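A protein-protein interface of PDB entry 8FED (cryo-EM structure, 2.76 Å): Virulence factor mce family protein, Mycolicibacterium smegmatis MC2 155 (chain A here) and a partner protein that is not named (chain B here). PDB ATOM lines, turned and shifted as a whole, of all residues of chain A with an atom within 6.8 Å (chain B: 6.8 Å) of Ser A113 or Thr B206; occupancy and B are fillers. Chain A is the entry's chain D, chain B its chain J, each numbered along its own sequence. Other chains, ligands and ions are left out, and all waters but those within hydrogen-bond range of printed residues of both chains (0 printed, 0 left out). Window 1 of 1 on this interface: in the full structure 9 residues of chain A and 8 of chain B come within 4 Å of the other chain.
A ring nitrogen (NE2) of His B209 lies close to the side-chain hydroxyl (OH) of Tyr A60, at 3.0 Å.
N of Gly B205 lies close to O of Pro A61, 3.5 Å away.
The side-chain carboxylate (OD1) of Asp A63 lies within hydrogen-bond range of the side-chain hydroxyl (OG) of Ser B203 (3.0 Å).
The side-chain carboxylate of Asp A63 lies within hydrogen-bond range of the side-chain hydroxyl of Thr B206 (2.9 Å).
OG of Ser A109 sits at hydrogen-bond distance from O of Val A111.
The backbone NH (N) of Tyr A60 lies within hydrogen-bond range of the side-chain carboxylate (OD2) of Asp A63 (3.3 Å).
The side-chain hydroxyl (OG) of Ser B203 lies within hydrogen-bond range of the side-chain hydroxyl (OG1) of Thr B206, at 2.7 Å.
Gly B205 touches Tyr A60 (CA to CB, 3.96 Å).
Ser B203 touches Gly A62 (CB to O, 3.4 Å).
Ser B203 touches Lys A64.
Ala B107 touches Val A111.
Phe B108 touches Val A111.
CA of Ala A112 touches CB of Ala B107, 3.95 Å away.
Ser B203 touches Ser A113 (OG to CB, 3.98 Å).
OG1 of Thr B206 touches CB of Ser A113, at 3.2 Å.
Of the printed residues of chain B, Ser A113 touches Ser B203 and Thr B206.
Of the printed residues of chain A, Thr B206 touches Asp A63 and Ser A113.
Of the printed residues of chain B, Asp A63 touches Ser B203 (3.0 Å) and Thr B206 (2.9 Å).
Printed residues of chain A within 4 Å of Ala B107: Val A111 (3.8 Å) and Ala A112 (3.95 Å).
Of the printed residues of chain B, Tyr A60 touches Gly B205 and His B209.
Of the printed residues of chain B, Ala A112 touches Ala B107.
Printed residues of chain A within 4 Å of Gly B205: Tyr A60 and Pro A61.
Phe B111 touches none of the printed residues of chain A.
The nearest printed residue of chain B that does not touch Lys A64 is Gln B202 (4.5 Å).
Of the 17 printed residues of chain A, 8 touch a printed residue of chain B.
Of the 15 printed residues of chain B, 6 touch a printed residue of chain A.
Among the printed residues, 12 pairs touch across the chains.
Among the printed residues, no Asp or Glu carboxylate lies within 4 Å of a Lys or Arg side-chain nitrogen of the other chain.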
ATOM      1  N   ALA A  58     -12.423 -10.690 -27.660  1.00  0.00           N
ATOM      2  CA  ALA A  58     -13.644  -9.889 -27.775  1.00  0.00           C
ATOM      3  C   ALA A  58     -13.360  -8.395 -27.661  1.00  0.00           C
ATOM      4  O   ALA A  58     -14.229  -7.614 -27.266  1.00  0.00           O
ATOM      5  CB  ALA A  58     -14.696 -10.314 -26.747  1.00  0.00           C
ATOM      6  N   LEU A  59     -12.143  -7.989 -28.005  1.00  0.00           N
ATOM      7  CA  LEU A  59     -11.761  -6.587 -28.076  1.00  0.00           C
ATOM      8  C   LEU A  59     -11.429  -6.261 -29.523  1.00  0.00           C
ATOM      9  O   LEU A  59     -10.626  -6.959 -30.149  1.00  0.00           O
ATOM     10  CB  LEU A  59     -10.571  -6.293 -27.165  1.00  0.00           C
ATOM     11  CG  LEU A  59     -10.235  -4.827 -26.911  1.00  0.00           C
ATOM     12  CD1 LEU A  59     -11.361  -4.170 -26.144  1.00  0.00           C
ATOM     13  CD2 LEU A  59      -8.924  -4.700 -26.159  1.00  0.00           C
ATOM     14  N   TYR A  60     -12.050  -5.218 -30.051  1.00  0.00           N
ATOM     15  CA  TYR A  60     -11.948  -4.855 -31.454  1.00  0.00           C
ATOM     16  C   TYR A  60     -11.576  -3.388 -31.574  1.00  0.00           C
ATOM     17  O   TYR A  60     -11.803  -2.607 -30.644  1.00  0.00           O
ATOM     18  CB  TYR A  60     -13.277  -5.119 -32.176  1.00  0.00           C
ATOM     19  CG  TYR A  60     -13.981  -6.363 -31.696  1.00  0.00           C
ATOM     20  CD1 TYR A  60     -13.606  -7.616 -32.154  1.00  0.00           C
ATOM     21  CD2 TYR A  60     -15.022  -6.283 -30.784  1.00  0.00           C
ATOM     22  CE1 TYR A  60     -14.245  -8.754 -31.715  1.00  0.00           C
ATOM     23  CE2 TYR A  60     -15.670  -7.414 -30.341  1.00  0.00           C
ATOM     24  CZ  TYR A  60     -15.277  -8.647 -30.809  1.00  0.00           C
ATOM     25  OH  TYR A  60     -15.921  -9.778 -30.366  1.00  0.00           O
ATOM     26  N   PRO A  61     -10.970  -2.986 -32.693  1.00  0.00           N
ATOM     27  CA  PRO A  61     -10.690  -1.561 -32.904  1.00  0.00           C
ATOM     28  C   PRO A  61     -11.972  -0.744 -32.882  1.00  0.00           C
ATOM     29  O   PRO A  61     -13.002  -1.153 -33.421  1.00  0.00           O
ATOM     30  CB  PRO A  61     -10.022  -1.530 -34.282  1.00  0.00           C
ATOM     31  CG  PRO A  61      -9.451  -2.891 -34.451  1.00  0.00           C
ATOM     32  CD  PRO A  61     -10.407  -3.820 -33.770  1.00  0.00           C
ATOM     33  N   GLY A  62     -11.899   0.426 -32.258  1.00  0.00           N
ATOM     34  CA  GLY A  62     -13.059   1.263 -32.056  1.00  0.00           C
ATOM     35  C   GLY A  62     -13.728   1.104 -30.708  1.00  0.00           C
ATOM     36  O   GLY A  62     -14.588   1.924 -30.366  1.00  0.00           O
ATOM     37  N   ASP A  63     -13.367   0.080 -29.939  1.00  0.00           N
ATOM     38  CA  ASP A  63     -13.925  -0.087 -28.605  1.00  0.00           C
ATOM     39  C   ASP A  63     -13.456   1.034 -27.686  1.00  0.00           C
ATOM     40  O   ASP A  63     -12.368   1.590 -27.851  1.00  0.00           O
ATOM     41  CB  ASP A  63     -13.538  -1.445 -28.022  1.00  0.00           C
ATOM     42  CG  ASP A  63     -14.483  -2.550 -28.448  1.00  0.00           C
ATOM     43  OD1 ASP A  63     -15.452  -2.256 -29.176  1.00  0.00           O
ATOM     44  OD2 ASP A  63     -14.264  -3.711 -28.049  1.00  0.00           O
ATOM     45  N   LYS A  64     -14.297   1.366 -26.713  1.00  0.00           N
ATOM     46  CA  LYS A  64     -14.070   2.545 -25.892  1.00  0.00           C
ATOM     47  C   LYS A  64     -12.947   2.318 -24.888  1.00  0.00           C
ATOM     48  O   LYS A  64     -12.699   1.199 -24.434  1.00  0.00           O
ATOM     49  CB  LYS A  64     -15.352   2.933 -25.157  1.00  0.00           C
ATOM     50  CG  LYS A  64     -16.569   3.050 -26.060  1.00  0.00           C
ATOM     51  CD  LYS A  64     -16.316   4.008 -27.210  1.00  0.00           C
ATOM     52  CE  LYS A  64     -17.506   4.063 -28.150  1.00  0.00           C
ATOM     53  NZ  LYS A  64     -17.256   4.966 -29.307  1.00  0.00           N
ATOM     54  N   ARG A  71     -15.850   7.339 -20.674  1.00  0.00           N
ATOM     55  CA  ARG A  71     -15.158   7.255 -21.956  1.00  0.00           C
ATOM     56  C   ARG A  71     -14.232   8.448 -22.148  1.00  0.00           C
ATOM     57  O   ARG A  71     -14.629   9.597 -21.938  1.00  0.00           O
ATOM     58  CB  ARG A  71     -16.171   7.194 -23.099  1.00  0.00           C
ATOM     59  CG  ARG A  71     -17.120   6.011 -23.044  1.00  0.00           C
ATOM     60  CD  ARG A  71     -18.087   6.034 -24.216  1.00  0.00           C
ATOM     61  NE  ARG A  71     -18.976   4.878 -24.221  1.00  0.00           N
ATOM     62  CZ  ARG A  71     -19.871   4.627 -25.165  1.00  0.00           C
ATOM     63  NH1 ARG A  71     -20.030   5.436 -26.200  1.00  0.00           N
ATOM     64  NH2 ARG A  71     -20.628   3.537 -25.071  1.00  0.00           N
ATOM     65  N   LEU A 106     -11.639  -4.907 -19.511  1.00  0.00           N
ATOM     66  CA  LEU A 106     -12.804  -5.163 -18.680  1.00  0.00           C
ATOM     67  C   LEU A 106     -13.975  -5.622 -19.534  1.00  0.00           C
ATOM     68  O   LEU A 106     -14.167  -5.140 -20.657  1.00  0.00           O
ATOM     69  CB  LEU A 106     -13.206  -3.917 -17.884  1.00  0.00           C
ATOM     70  CG  LEU A 106     -12.175  -3.380 -16.892  1.00  0.00           C
ATOM     71  CD1 LEU A 106     -12.703  -2.139 -16.207  1.00  0.00           C
ATOM     72  CD2 LEU A 106     -11.812  -4.443 -15.870  1.00  0.00           C
ATOM     73  N   ASN A 107     -14.753  -6.553 -18.987  1.00  0.00           N
ATOM     74  CA  ASN A 107     -16.001  -7.017 -19.581  1.00  0.00           C
ATOM     75  C   ASN A 107     -17.138  -6.564 -18.675  1.00  0.00           C
ATOM     76  O   ASN A 107     -17.401  -7.205 -17.647  1.00  0.00           O
ATOM     77  CB  ASN A 107     -16.002  -8.540 -19.734  1.00  0.00           C
ATOM     78  CG  ASN A 107     -17.250  -9.057 -20.416  1.00  0.00           C
ATOM     79  OD1 ASN A 107     -17.957  -8.310 -21.090  1.00  0.00           O
ATOM     80  ND2 ASN A 107     -17.524 -10.344 -20.249  1.00  0.00           N
ATOM     81  N   PRO A 108     -17.822  -5.459 -18.998  1.00  0.00           N
ATOM     82  CA  PRO A 108     -18.757  -4.856 -18.030  1.00  0.00           C
ATOM     83  C   PRO A 108     -19.900  -5.757 -17.590  1.00  0.00           C
ATOM     84  O   PRO A 108     -20.305  -5.693 -16.423  1.00  0.00           O
ATOM     85  CB  PRO A 108     -19.271  -3.619 -18.780  1.00  0.00           C
ATOM     86  CG  PRO A 108     -18.192  -3.297 -19.756  1.00  0.00           C
ATOM     87  CD  PRO A 108     -17.655  -4.623 -20.198  1.00  0.00           C
ATOM     88  N   SER A 109     -20.438  -6.592 -18.474  1.00  0.00           N
ATOM     89  CA  SER A 109     -21.593  -7.404 -18.117  1.00  0.00           C
ATOM     90  C   SER A 109     -21.550  -8.701 -18.912  1.00  0.00           C
ATOM     91  O   SER A 109     -20.538  -9.034 -19.535  1.00  0.00           O
ATOM     92  CB  SER A 109     -22.894  -6.625 -18.347  1.00  0.00           C
ATOM     93  OG  SER A 109     -23.054  -6.283 -19.711  1.00  0.00           O
ATOM     94  N   VAL A 111     -23.281  -9.653 -21.671  1.00  0.00           N
ATOM     95  CA  VAL A 111     -23.151  -9.338 -23.087  1.00  0.00           C
ATOM     96  C   VAL A 111     -22.883  -7.844 -23.183  1.00  0.00           C
ATOM     97  O   VAL A 111     -23.799  -7.026 -23.031  1.00  0.00           O
ATOM     98  CB  VAL A 111     -24.395  -9.730 -23.889  1.00  0.00           C
ATOM     99  CG1 VAL A 111     -24.228  -9.326 -25.340  1.00  0.00           C
ATOM    100  CG2 VAL A 111     -24.654 -11.222 -23.770  1.00  0.00           C
ATOM    101  N   ALA A 112     -21.631  -7.479 -23.436  1.00  0.00           N
ATOM    102  CA  ALA A 112     -21.249  -6.080 -23.527  1.00  0.00           C
ATOM    103  C   ALA A 112     -20.015  -5.965 -24.405  1.00  0.00           C
ATOM    104  O   ALA A 112     -19.417  -6.964 -24.813  1.00  0.00           O
ATOM    105  CB  ALA A 112     -20.989  -5.478 -22.144  1.00  0.00           C
ATOM    106  N   SER A 113     -19.642  -4.725 -24.702  1.00  0.00           N
ATOM    107  CA  SER A 113     -18.430  -4.439 -25.452  1.00  0.00           C
ATOM    108  C   SER A 113     -17.284  -4.251 -24.466  1.00  0.00           C
ATOM    109  O   SER A 113     -17.330  -3.346 -23.625  1.00  0.00           O
ATOM    110  CB  SER A 113     -18.609  -3.196 -26.322  1.00  0.00           C
ATOM    111  OG  SER A 113     -18.868  -2.051 -25.531  1.00  0.00           O
ATOM    112  N   ARG A 114     -16.274  -5.110 -24.557  1.00  0.00           N
ATOM    113  CA  ARG A 114     -15.136  -5.019 -23.656  1.00  0.00           C
ATOM    114  C   ARG A 114     -14.372  -3.724 -23.893  1.00  0.00           C
ATOM    115  O   ARG A 114     -14.290  -3.220 -25.015  1.00  0.00           O
ATOM    116  CB  ARG A 114     -14.213  -6.221 -23.833  1.00  0.00           C
ATOM    117  CG  ARG A 114     -14.919  -7.551 -23.671  1.00  0.00           C
ATOM    118  CD  ARG A 114     -13.933  -8.680 -23.472  1.00  0.00           C
ATOM    119  NE  ARG A 114     -14.607  -9.961 -23.314  1.00  0.00           N
ATOM    120  CZ  ARG A 114     -14.005 -11.085 -22.954  1.00  0.00           C
ATOM    121  NH1 ARG A 114     -12.709 -11.121 -22.697  1.00  0.00           N
ATOM    122  NH2 ARG A 114     -14.721 -12.199 -22.845  1.00  0.00           N
ATOM    123  N   VAL A 115     -13.819  -3.176 -22.814  1.00  0.00           N
ATOM    124  CA  VAL A 115     -13.155  -1.882 -22.848  1.00  0.00           C
ATOM    125  C   VAL A 115     -11.758  -2.026 -22.260  1.00  0.00           C
ATOM    126  O   VAL A 115     -11.405  -3.054 -21.687  1.00  0.00           O
ATOM    127  CB  VAL A 115     -13.947  -0.806 -22.081  1.00  0.00           C
ATOM    128  CG1 VAL A 115     -15.307  -0.590 -22.717  1.00  0.00           C
ATOM    129  CG2 VAL A 115     -14.098  -1.217 -20.631  1.00  0.00           C
ATOM    130  N   GLU B 106     -27.365  -5.292 -25.040  1.00  0.00           N
ATOM    131  CA  GLU B 106     -27.433  -4.342 -26.144  1.00  0.00           C
ATOM    132  C   GLU B 106     -26.268  -4.459 -27.118  1.00  0.00           C
ATOM    133  O   GLU B 106     -26.250  -3.742 -28.122  1.00  0.00           O
ATOM    134  CB  GLU B 106     -27.502  -2.911 -25.602  1.00  0.00           C
ATOM    135  CG  GLU B 106     -26.339  -2.539 -24.704  1.00  0.00           C
ATOM    136  CD  GLU B 106     -26.514  -1.182 -24.057  1.00  0.00           C
ATOM    137  OE1 GLU B 106     -27.505  -0.493 -24.375  1.00  0.00           O
ATOM    138  OE2 GLU B 106     -25.659  -0.804 -23.229  1.00  0.00           O
ATOM    139  N   ALA B 107     -25.301  -5.336 -26.853  1.00  0.00           N
ATOM    140  CA  ALA B 107     -24.201  -5.540 -27.788  1.00  0.00           C
ATOM    141  C   ALA B 107     -24.590  -6.413 -28.971  1.00  0.00           C
ATOM    142  O   ALA B 107     -23.821  -6.501 -29.934  1.00  0.00           O
ATOM    143  CB  ALA B 107     -23.003  -6.155 -27.066  1.00  0.00           C
ATOM    144  N   PHE B 108     -25.755  -7.050 -28.926  1.00  0.00           N
ATOM    145  CA  PHE B 108     -26.239  -7.902 -30.003  1.00  0.00           C
ATOM    146  C   PHE B 108     -26.961  -7.131 -31.098  1.00  0.00           C
ATOM    147  O   PHE B 108     -27.426  -7.754 -32.060  1.00  0.00           O
ATOM    148  CB  PHE B 108     -27.177  -8.975 -29.442  1.00  0.00           C
ATOM    149  CG  PHE B 108     -26.476 -10.073 -28.696  1.00  0.00           C
ATOM    150  CD1 PHE B 108     -25.134 -10.328 -28.910  1.00  0.00           C
ATOM    151  CD2 PHE B 108     -27.167 -10.861 -27.793  1.00  0.00           C
ATOM    152  CE1 PHE B 108     -24.491 -11.346 -28.231  1.00  0.00           C
ATOM    153  CE2 PHE B 108     -26.530 -11.877 -27.110  1.00  0.00           C
ATOM    154  CZ  PHE B 108     -25.190 -12.119 -27.330  1.00  0.00           C
ATOM    155  N   GLY B 110     -26.336  -5.162 -33.725  1.00  0.00           N
ATOM    156  CA  GLY B 110     -25.980  -5.445 -35.105  1.00  0.00           C
ATOM    157  C   GLY B 110     -26.380  -6.845 -35.519  1.00  0.00           C
ATOM    158  O   GLY B 110     -27.013  -7.042 -36.561  1.00  0.00           O
ATOM    159  N   PHE B 111     -26.058  -7.833 -34.675  1.00  0.00           N
ATOM    160  CA  PHE B 111     -26.444  -9.213 -34.948  1.00  0.00           C
ATOM    161  C   PHE B 111     -27.948  -9.336 -35.138  1.00  0.00           C
ATOM    162  O   PHE B 111     -28.411 -10.168 -35.927  1.00  0.00           O
ATOM    163  CB  PHE B 111     -25.957 -10.119 -33.813  1.00  0.00           C
ATOM    164  CG  PHE B 111     -26.968 -11.133 -33.359  1.00  0.00           C
ATOM    165  CD1 PHE B 111     -27.139 -12.320 -34.044  1.00  0.00           C
ATOM    166  CD2 PHE B 111     -27.740 -10.902 -32.235  1.00  0.00           C
ATOM    167  CE1 PHE B 111     -28.068 -13.241 -33.624  1.00  0.00           C
ATOM    168  CE2 PHE B 111     -28.670 -11.826 -31.810  1.00  0.00           C
ATOM    169  CZ  PHE B 111     -28.831 -12.998 -32.506  1.00  0.00           C
ATOM    170  N   GLN B 202     -22.649   3.530 -29.922  1.00  0.00           N
ATOM    171  CA  GLN B 202     -22.060   2.210 -29.760  1.00  0.00           C
ATOM    172  C   GLN B 202     -20.744   2.132 -30.525  1.00  0.00           C
ATOM    173  O   GLN B 202     -20.565   2.779 -31.560  1.00  0.00           O
ATOM    174  CB  GLN B 202     -23.018   1.120 -30.247  1.00  0.00           C
ATOM    175  CG  GLN B 202     -22.585  -0.291 -29.871  1.00  0.00           C
ATOM    176  CD  GLN B 202     -23.536  -1.357 -30.367  1.00  0.00           C
ATOM    177  OE1 GLN B 202     -23.685  -1.561 -31.569  1.00  0.00           O
ATOM    178  NE2 GLN B 202     -24.180  -2.051 -29.438  1.00  0.00           N
ATOM    179  N   SER B 203     -19.808   1.349 -29.989  1.00  0.00           N
ATOM    180  CA  SER B 203     -18.517   1.180 -30.640  1.00  0.00           C
ATOM    181  C   SER B 203     -18.690   0.507 -31.995  1.00  0.00           C
ATOM    182  O   SER B 203     -19.459  -0.447 -32.140  1.00  0.00           O
ATOM    183  CB  SER B 203     -17.579   0.359 -29.757  1.00  0.00           C
ATOM    184  OG  SER B 203     -18.081  -0.951 -29.566  1.00  0.00           O
ATOM    185  N   VAL B 204     -17.970   1.019 -32.996  1.00  0.00           N
ATOM    186  CA  VAL B 204     -18.092   0.482 -34.346  1.00  0.00           C
ATOM    187  C   VAL B 204     -17.507  -0.923 -34.434  1.00  0.00           C
ATOM    188  O   VAL B 204     -17.989  -1.753 -35.214  1.00  0.00           O
ATOM    189  CB  VAL B 204     -17.443   1.450 -35.358  1.00  0.00           C
ATOM    190  CG1 VAL B 204     -15.962   1.642 -35.063  1.00  0.00           C
ATOM    191  CG2 VAL B 204     -17.661   0.973 -36.786  1.00  0.00           C
ATOM    192  N   GLY B 205     -16.478  -1.225 -33.636  1.00  0.00           N
ATOM    193  CA  GLY B 205     -15.869  -2.544 -33.694  1.00  0.00           C
ATOM    194  C   GLY B 205     -16.808  -3.654 -33.263  1.00  0.00           C
ATOM    195  O   GLY B 205     -16.886  -4.699 -33.913  1.00  0.00           O
ATOM    196  N   THR B 206     -17.534  -3.441 -32.162  1.00  0.00           N
ATOM    197  CA  THR B 206     -18.497  -4.434 -31.698  1.00  0.00           C
ATOM    198  C   THR B 206     -19.606  -4.645 -32.719  1.00  0.00           C
ATOM    199  O   THR B 206     -20.010  -5.786 -32.987  1.00  0.00           O
ATOM    200  CB  THR B 206     -19.082  -3.998 -30.356  1.00  0.00           C
ATOM    201  OG1 THR B 206     -18.016  -3.670 -29.458  1.00  0.00           O
ATOM    202  CG2 THR B 206     -19.916  -5.105 -29.749  1.00  0.00           C
ATOM    203  N   TYR B 207     -20.112  -3.552 -33.295  1.00  0.00           N
ATOM    204  CA  TYR B 207     -21.165  -3.655 -34.298  1.00  0.00           C
ATOM    205  C   TYR B 207     -20.680  -4.427 -35.514  1.00  0.00           C
ATOM    206  O   TYR B 207     -21.381  -5.306 -36.024  1.00  0.00           O
ATOM    207  CB  TYR B 207     -21.649  -2.260 -34.701  1.00  0.00           C
ATOM    208  CG  TYR B 207     -22.865  -2.268 -35.605  1.00  0.00           C
ATOM    209  CD1 TYR B 207     -22.736  -2.400 -36.981  1.00  0.00           C
ATOM    210  CD2 TYR B 207     -24.143  -2.139 -35.081  1.00  0.00           C
ATOM    211  CE1 TYR B 207     -23.839  -2.413 -37.804  1.00  0.00           C
ATOM    212  CE2 TYR B 207     -25.253  -2.145 -35.899  1.00  0.00           C
ATOM    213  CZ  TYR B 207     -25.095  -2.284 -37.258  1.00  0.00           C
ATOM    214  OH  TYR B 207     -26.198  -2.294 -38.078  1.00  0.00           O
ATOM    215  N   GLU B 208     -19.474  -4.113 -35.995  1.00  0.00           N
ATOM    216  CA  GLU B 208     -18.940  -4.808 -37.161  1.00  0.00           C
ATOM    217  C   GLU B 208     -18.699  -6.282 -36.866  1.00  0.00           C
ATOM    218  O   GLU B 208     -18.954  -7.137 -37.722  1.00  0.00           O
ATOM    219  CB  GLU B 208     -17.654  -4.136 -37.636  1.00  0.00           C
ATOM    220  CG  GLU B 208     -17.869  -2.776 -38.277  1.00  0.00           C
ATOM    221  CD  GLU B 208     -16.580  -2.162 -38.782  1.00  0.00           C
ATOM    222  OE1 GLU B 208     -15.506  -2.753 -38.543  1.00  0.00           O
ATOM    223  OE2 GLU B 208     -16.640  -1.090 -39.419  1.00  0.00           O
ATOM    224  N   HIS B 209     -18.208  -6.600 -35.665  1.00  0.00           N
ATOM    225  CA  HIS B 209     -17.986  -7.996 -35.303  1.00  0.00           C
ATOM    226  C   HIS B 209     -19.293  -8.775 -35.292  1.00  0.00           C
ATOM    227  O   HIS B 209     -19.403  -9.834 -35.922  1.00  0.00           O
ATOM    228  CB  HIS B 209     -17.303  -8.086 -33.942  1.00  0.00           C
ATOM    229  CG  HIS B 209     -17.148  -9.487 -33.441  1.00  0.00           C
ATOM    230  ND1 HIS B 209     -16.109 -10.306 -33.824  1.00  0.00           N
ATOM    231  CD2 HIS B 209     -17.912 -10.221 -32.596  1.00  0.00           C
ATOM    232  CE1 HIS B 209     -16.232 -11.478 -33.230  1.00  0.00           C
ATOM    233  NE2 HIS B 209     -17.318 -11.453 -32.480  1.00  0.00           N
ATOM    234  N   TYR B 210     -20.306  -8.258 -34.595  1.00  0.00           N
ATOM    235  CA  TYR B 210     -21.574  -8.976 -34.521  1.00  0.00           C
ATOM    236  C   TYR B 210     -22.348  -8.922 -35.831  1.00  0.00           C
ATOM    237  O   TYR B 210     -23.270  -9.720 -36.023  1.00  0.00           O
ATOM    238  CB  TYR B 210     -22.425  -8.435 -33.374  1.00  0.00           C
ATOM    239  CG  TYR B 210     -21.975  -8.930 -32.020  1.00  0.00           C
ATOM    240  CD1 TYR B 210     -22.265 -10.220 -31.602  1.00  0.00           C
ATOM    241  CD2 TYR B 210     -21.255  -8.112 -31.163  1.00  0.00           C
ATOM    242  CE1 TYR B 210     -21.854 -10.680 -30.371  1.00  0.00           C
ATOM    243  CE2 TYR B 210     -20.839  -8.563 -29.929  1.00  0.00           C
ATOM    244  CZ  TYR B 210     -21.143  -9.847 -29.538  1.00  0.00           C
ATOM    245  OH  TYR B 210     -20.730 -10.302 -28.306  1.00  0.00           O
ATOM    246  N   PHE B 211     -21.991  -8.008 -36.733  1.00  0.00           N
ATOM    247  CA  PHE B 211     -22.638  -7.941 -38.036  1.00  0.00           C
ATOM    248  C   PHE B 211     -22.037  -8.959 -38.997  1.00  0.00           C
ATOM    249  O   PHE B 211     -22.762  -9.736 -39.623  1.00  0.00           O
ATOM    250  CB  PHE B 211     -22.518  -6.518 -38.593  1.00  0.00           C
ATOM    251  CG  PHE B 211     -23.068  -6.352 -39.982  1.00  0.00           C
ATOM    252  CD1 PHE B 211     -24.417  -6.140 -40.184  1.00  0.00           C
ATOM    253  CD2 PHE B 211     -22.229  -6.379 -41.082  1.00  0.00           C
ATOM    254  CE1 PHE B 211     -24.923  -5.981 -41.457  1.00  0.00           C
ATOM    255  CE2 PHE B 211     -22.731  -6.222 -42.357  1.00  0.00           C
ATOM    256  CZ  PHE B 211     -24.078  -6.021 -42.543  1.00  0.00           C
